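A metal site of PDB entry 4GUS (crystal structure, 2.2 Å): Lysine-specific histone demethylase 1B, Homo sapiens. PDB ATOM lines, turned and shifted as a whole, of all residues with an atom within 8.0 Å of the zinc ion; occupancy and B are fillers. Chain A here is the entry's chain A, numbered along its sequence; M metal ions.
The zinc ion is bound by SG of Cys 123, SG of Cys 101, SG of Cys 96 and SG of Cys 139. The zinc ion has four donor atoms within binding distance.
The nearest printed residue that does not touch the zinc ion is Lys 98 (4.8 Å).
The guanidinium group (NH1) of Arg 105 lies close to the side-chain sulfur (SG) of Cys 123, 3.3 Å away. The side-chain sulfur of Cys 101 sits close to the backbone NH of Lys 103 (3.5 Å). The backbone NH (N) of Lys 98 sits close to the side-chain sulfur (SG) of Cys 96, at 3.4 Å. The backbone carbonyl oxygen (O) of Cys 96 sits at hydrogen-bond distance from the guanidinium group (NH2) of Arg 102. N of Cys 96 lies within hydrogen-bond range of O of Lys 103 (2.8 Å). The side-chain amino group of Lys 103 sits close to the backbone carbonyl oxygen of Cys 139 (3.2 Å).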
ATOM      1  N   GLN A  95      11.023  -9.011  29.312  1.00  0.00           N
ATOM      2  CA  GLN A  95      11.550  -9.197  27.962  1.00  0.00           C
ATOM      3  C   GLN A  95      11.620 -10.673  27.570  1.00  0.00           C
ATOM      4  O   GLN A  95      11.988 -11.507  28.390  1.00  0.00           O
ATOM      5  CB  GLN A  95      12.926  -8.545  27.841  1.00  0.00           C
ATOM      6  CG  GLN A  95      13.315  -8.173  26.404  1.00  0.00           C
ATOM      7  CD  GLN A  95      14.637  -7.406  26.316  1.00  0.00           C
ATOM      8  OE1 GLN A  95      15.302  -7.131  27.326  1.00  0.00           O
ATOM      9  NE2 GLN A  95      15.029  -7.048  25.084  1.00  0.00           N
ATOM     10  N   CYS A  96      11.268 -10.982  26.332  1.00  0.00           N
ATOM     11  CA  CYS A  96      11.311 -12.350  25.838  1.00  0.00           C
ATOM     12  C   CYS A  96      12.741 -12.862  25.751  1.00  0.00           C
ATOM     13  O   CYS A  96      13.635 -12.170  25.278  1.00  0.00           O
ATOM     14  CB  CYS A  96      10.650 -12.469  24.462  1.00  0.00           C
ATOM     15  SG  CYS A  96      10.821 -14.111  23.714  1.00  0.00           S
ATOM     16  N   THR A  97      12.906 -14.111  26.195  1.00  0.00           N
ATOM     17  CA  THR A  97      14.208 -14.757  26.364  1.00  0.00           C
ATOM     18  C   THR A  97      14.781 -15.313  25.057  1.00  0.00           C
ATOM     19  O   THR A  97      15.998 -15.502  24.931  1.00  0.00           O
ATOM     20  CB  THR A  97      14.092 -15.853  27.470  1.00  0.00           C
ATOM     21  OG1 THR A  97      14.145 -15.212  28.755  1.00  0.00           O
ATOM     22  CG2 THR A  97      15.171 -16.923  27.374  1.00  0.00           C
ATOM     23  N   LYS A  98      13.912 -15.567  24.079  1.00  0.00           N
ATOM     24  CA  LYS A  98      14.371 -16.024  22.780  1.00  0.00           C
ATOM     25  C   LYS A  98      15.312 -15.006  22.143  1.00  0.00           C
ATOM     26  O   LYS A  98      14.968 -13.823  21.998  1.00  0.00           O
ATOM     27  CB  LYS A  98      13.193 -16.328  21.847  1.00  0.00           C
ATOM     28  CG  LYS A  98      12.417 -17.582  22.211  1.00  0.00           C
ATOM     29  CD  LYS A  98      11.619 -18.107  21.023  1.00  0.00           C
ATOM     30  CE  LYS A  98      10.868 -19.382  21.392  1.00  0.00           C
ATOM     31  NZ  LYS A  98      10.115 -19.955  20.236  1.00  0.00           N
ATOM     32  N   PRO A  99      16.521 -15.462  21.769  1.00  0.00           N
ATOM     33  CA  PRO A  99      17.557 -14.617  21.167  1.00  0.00           C
ATOM     34  C   PRO A  99      17.138 -13.933  19.858  1.00  0.00           C
ATOM     35  O   PRO A  99      17.541 -12.798  19.611  1.00  0.00           O
ATOM     36  CB  PRO A  99      18.702 -15.611  20.913  1.00  0.00           C
ATOM     37  CG  PRO A  99      18.494 -16.680  21.960  1.00  0.00           C
ATOM     38  CD  PRO A  99      17.010 -16.818  22.065  1.00  0.00           C
ATOM     39  N   GLU A 100      16.336 -14.618  19.050  1.00  0.00           N
ATOM     40  CA  GLU A 100      15.888 -14.067  17.771  1.00  0.00           C
ATOM     41  C   GLU A 100      14.687 -13.123  17.898  1.00  0.00           C
ATOM     42  O   GLU A 100      14.286 -12.479  16.921  1.00  0.00           O
ATOM     43  CB  GLU A 100      15.589 -15.200  16.772  1.00  0.00           C
ATOM     44  CG  GLU A 100      14.541 -16.208  17.249  1.00  0.00           C
ATOM     45  CD  GLU A 100      15.123 -17.316  18.125  1.00  0.00           C
ATOM     46  OE1 GLU A 100      14.440 -18.355  18.288  1.00  0.00           O
ATOM     47  OE2 GLU A 100      16.237 -17.156  18.663  1.00  0.00           O
ATOM     48  N   CYS A 101      14.109 -13.057  19.096  1.00  0.00           N
ATOM     49  CA  CYS A 101      12.925 -12.214  19.344  1.00  0.00           C
ATOM     50  C   CYS A 101      13.257 -11.026  20.246  1.00  0.00           C
ATOM     51  O   CYS A 101      13.317  -9.895  19.777  1.00  0.00           O
ATOM     52  CB  CYS A 101      11.805 -13.047  19.958  1.00  0.00           C
ATOM     53  SG  CYS A 101      10.442 -12.086  20.611  1.00  0.00           S
ATOM     54  N   ARG A 102      13.462 -11.294  21.535  1.00  0.00           N
ATOM     55  CA  ARG A 102      13.854 -10.270  22.509  1.00  0.00           C
ATOM     56  C   ARG A 102      12.858  -9.112  22.690  1.00  0.00           C
ATOM     57  O   ARG A 102      13.243  -8.041  23.138  1.00  0.00           O
ATOM     58  CB  ARG A 102      15.252  -9.732  22.179  1.00  0.00           C
ATOM     59  CG  ARG A 102      16.376 -10.790  22.236  1.00  0.00           C
ATOM     60  CD  ARG A 102      16.566 -11.319  23.658  1.00  0.00           C
ATOM     61  NE  ARG A 102      17.139 -10.293  24.519  1.00  0.00           N
ATOM     62  CZ  ARG A 102      16.950 -10.217  25.845  1.00  0.00           C
ATOM     63  NH1 ARG A 102      17.522  -9.239  26.523  1.00  0.00           N
ATOM     64  NH2 ARG A 102      16.186 -11.110  26.468  1.00  0.00           N
ATOM     65  N   LYS A 103      11.592  -9.333  22.346  1.00  0.00           N
ATOM     66  CA  LYS A 103      10.571  -8.291  22.471  1.00  0.00           C
ATOM     67  C   LYS A 103      10.106  -8.068  23.912  1.00  0.00           C
ATOM     68  O   LYS A 103      10.099  -8.999  24.721  1.00  0.00           O
ATOM     69  CB  LYS A 103       9.353  -8.627  21.606  1.00  0.00           C
ATOM     70  CG  LYS A 103       9.657  -8.752  20.123  1.00  0.00           C
ATOM     71  CD  LYS A 103       8.401  -9.093  19.343  1.00  0.00           C
ATOM     72  CE  LYS A 103       8.672  -9.087  17.858  1.00  0.00           C
ATOM     73  NZ  LYS A 103       7.404  -9.003  17.104  1.00  0.00           N
ATOM     74  N   TRP A 104       9.705  -6.840  24.212  1.00  0.00           N
ATOM     75  CA  TRP A 104       9.146  -6.484  25.513  1.00  0.00           C
ATOM     76  C   TRP A 104       7.626  -6.690  25.558  1.00  0.00           C
ATOM     77  O   TRP A 104       6.903  -6.255  24.653  1.00  0.00           O
ATOM     78  CB  TRP A 104       9.466  -5.033  25.840  1.00  0.00           C
ATOM     79  CG  TRP A 104      10.856  -4.841  26.382  1.00  0.00           C
ATOM     80  CD1 TRP A 104      11.978  -4.485  25.677  1.00  0.00           C
ATOM     81  CD2 TRP A 104      11.272  -5.002  27.745  1.00  0.00           C
ATOM     82  NE1 TRP A 104      13.076  -4.404  26.528  1.00  0.00           N
ATOM     83  CE2 TRP A 104      12.664  -4.723  27.797  1.00  0.00           C
ATOM     84  CE3 TRP A 104      10.614  -5.376  28.917  1.00  0.00           C
ATOM     85  CZ2 TRP A 104      13.391  -4.790  28.980  1.00  0.00           C
ATOM     86  CZ3 TRP A 104      11.325  -5.435  30.089  1.00  0.00           C
ATOM     87  CH2 TRP A 104      12.706  -5.156  30.120  1.00  0.00           C
ATOM     88  N   ARG A 105       7.142  -7.327  26.628  1.00  0.00           N
ATOM     89  CA  ARG A 105       5.721  -7.631  26.742  1.00  0.00           C
ATOM     90  C   ARG A 105       5.180  -7.172  28.079  1.00  0.00           C
ATOM     91  O   ARG A 105       5.879  -7.232  29.101  1.00  0.00           O
ATOM     92  CB  ARG A 105       5.441  -9.129  26.545  1.00  0.00           C
ATOM     93  CG  ARG A 105       6.311  -9.817  25.512  1.00  0.00           C
ATOM     94  CD  ARG A 105       5.539 -10.325  24.283  1.00  0.00           C
ATOM     95  NE  ARG A 105       5.168  -9.242  23.380  1.00  0.00           N
ATOM     96  CZ  ARG A 105       5.085  -9.341  22.052  1.00  0.00           C
ATOM     97  NH1 ARG A 105       5.347 -10.478  21.420  1.00  0.00           N
ATOM     98  NH2 ARG A 105       4.739  -8.267  21.348  1.00  0.00           N
ATOM     99  N   TYR A 121      11.262 -16.049  30.875  1.00  0.00           N
ATOM    100  CA  TYR A 121      10.060 -15.612  30.153  1.00  0.00           C
ATOM    101  C   TYR A 121      10.135 -15.792  28.625  1.00  0.00           C
ATOM    102  O   TYR A 121      11.172 -15.576  28.020  1.00  0.00           O
ATOM    103  CB  TYR A 121       9.738 -14.156  30.484  1.00  0.00           C
ATOM    104  CG  TYR A 121       8.506 -13.662  29.756  1.00  0.00           C
ATOM    105  CD1 TYR A 121       8.622 -12.936  28.569  1.00  0.00           C
ATOM    106  CD2 TYR A 121       7.227 -13.928  30.242  1.00  0.00           C
ATOM    107  CE1 TYR A 121       7.505 -12.499  27.901  1.00  0.00           C
ATOM    108  CE2 TYR A 121       6.109 -13.492  29.574  1.00  0.00           C
ATOM    109  CZ  TYR A 121       6.239 -12.787  28.408  1.00  0.00           C
ATOM    110  OH  TYR A 121       5.121 -12.350  27.740  1.00  0.00           O
ATOM    111  N   ARG A 122       9.021 -16.197  28.028  1.00  0.00           N
ATOM    112  CA  ARG A 122       8.915 -16.266  26.570  1.00  0.00           C
ATOM    113  C   ARG A 122       7.552 -15.698  26.167  1.00  0.00           C
ATOM    114  O   ARG A 122       6.605 -15.770  26.945  1.00  0.00           O
ATOM    115  CB  ARG A 122       9.047 -17.698  26.053  1.00  0.00           C
ATOM    116  CG  ARG A 122      10.309 -18.405  26.505  1.00  0.00           C
ATOM    117  CD  ARG A 122      10.999 -19.147  25.376  1.00  0.00           C
ATOM    118  NE  ARG A 122      12.376 -19.467  25.748  1.00  0.00           N
ATOM    119  CZ  ARG A 122      13.241 -20.118  24.971  1.00  0.00           C
ATOM    120  NH1 ARG A 122      12.859 -20.537  23.763  1.00  0.00           N
ATOM    121  NH2 ARG A 122      14.474 -20.346  25.403  1.00  0.00           N
ATOM    122  N   CYS A 123       7.481 -15.136  24.958  1.00  0.00           N
ATOM    123  CA  CYS A 123       6.247 -14.538  24.442  1.00  0.00           C
ATOM    124  C   CYS A 123       5.039 -15.464  24.569  1.00  0.00           C
ATOM    125  O   CYS A 123       5.046 -16.564  24.032  1.00  0.00           O
ATOM    126  CB  CYS A 123       6.417 -14.113  22.989  1.00  0.00           C
ATOM    127  SG  CYS A 123       7.471 -12.668  22.747  1.00  0.00           S
ATOM    128  N   GLY A 124       4.016 -15.006  25.282  1.00  0.00           N
ATOM    129  CA  GLY A 124       2.762 -15.725  25.390  1.00  0.00           C
ATOM    130  C   GLY A 124       2.774 -16.893  26.360  1.00  0.00           C
ATOM    131  O   GLY A 124       1.982 -17.827  26.215  1.00  0.00           O
ATOM    132  N   ASP A 137       2.537 -18.686  16.738  1.00  0.00           N
ATOM    133  CA  ASP A 137       3.880 -18.227  17.086  1.00  0.00           C
ATOM    134  C   ASP A 137       3.781 -16.855  17.752  1.00  0.00           C
ATOM    135  O   ASP A 137       3.632 -15.840  17.070  1.00  0.00           O
ATOM    136  CB  ASP A 137       4.741 -18.133  15.833  1.00  0.00           C
ATOM    137  CG  ASP A 137       6.071 -17.465  16.100  1.00  0.00           C
ATOM    138  OD1 ASP A 137       6.664 -17.718  17.173  1.00  0.00           O
ATOM    139  OD2 ASP A 137       6.520 -16.676  15.232  1.00  0.00           O
ATOM    140  N   HIS A 138       3.869 -16.823  19.078  1.00  0.00           N
ATOM    141  CA  HIS A 138       3.636 -15.589  19.818  1.00  0.00           C
ATOM    142  C   HIS A 138       4.752 -14.553  19.716  1.00  0.00           C
ATOM    143  O   HIS A 138       4.546 -13.384  20.038  1.00  0.00           O
ATOM    144  CB  HIS A 138       3.325 -15.902  21.270  1.00  0.00           C
ATOM    145  CG  HIS A 138       2.096 -16.738  21.439  1.00  0.00           C
ATOM    146  ND1 HIS A 138       0.835 -16.199  21.485  1.00  0.00           N
ATOM    147  CD2 HIS A 138       1.950 -18.074  21.554  1.00  0.00           C
ATOM    148  CE1 HIS A 138      -0.048 -17.171  21.636  1.00  0.00           C
ATOM    149  NE2 HIS A 138       0.606 -18.320  21.683  1.00  0.00           N
ATOM    150  N   CYS A 139       5.938 -14.973  19.290  1.00  0.00           N
ATOM    151  CA  CYS A 139       7.065 -14.056  19.174  1.00  0.00           C
ATOM    152  C   CYS A 139       6.921 -13.088  18.006  1.00  0.00           C
ATOM    153  O   CYS A 139       7.548 -12.031  18.006  1.00  0.00           O
ATOM    154  CB  CYS A 139       8.375 -14.836  19.044  1.00  0.00           C
ATOM    155  SG  CYS A 139       8.870 -15.661  20.567  1.00  0.00           S
ATOM    156  N   SER A 140       6.096 -13.451  17.015  1.00  0.00           N
ATOM    157  CA  SER A 140       5.881 -12.631  15.829  1.00  0.00           C
ATOM    158  C   SER A 140       4.820 -11.554  16.054  1.00  0.00           C
ATOM    159  O   SER A 140       4.684 -10.633  15.246  1.00  0.00           O
ATOM    160  CB  SER A 140       5.491 -13.490  14.629  1.00  0.00           C
ATOM    161  OG  SER A 140       4.216 -14.087  14.820  1.00  0.00           O
ATOM    162  N   LEU A 141       4.070 -11.685  17.148  1.00  0.00           N
ATOM    163  CA  LEU A 141       3.154 -10.651  17.587  1.00  0.00           C
ATOM    164  C   LEU A 141       3.882  -9.312  17.703  1.00  0.00           C
ATOM    165  O   LEU A 141       5.009  -9.258  18.217  1.00  0.00           O
ATOM    166  CB  LEU A 141       2.538 -11.009  18.935  1.00  0.00           C
ATOM    167  CG  LEU A 141       1.375 -12.001  18.951  1.00  0.00           C
ATOM    168  CD1 LEU A 141       1.233 -12.624  20.344  1.00  0.00           C
ATOM    169  CD2 LEU A 141       0.079 -11.307  18.535  1.00  0.00           C
HETATM  170 ZN    ZN M   1       9.259 -13.658  21.942  1.00  0.00          ZN
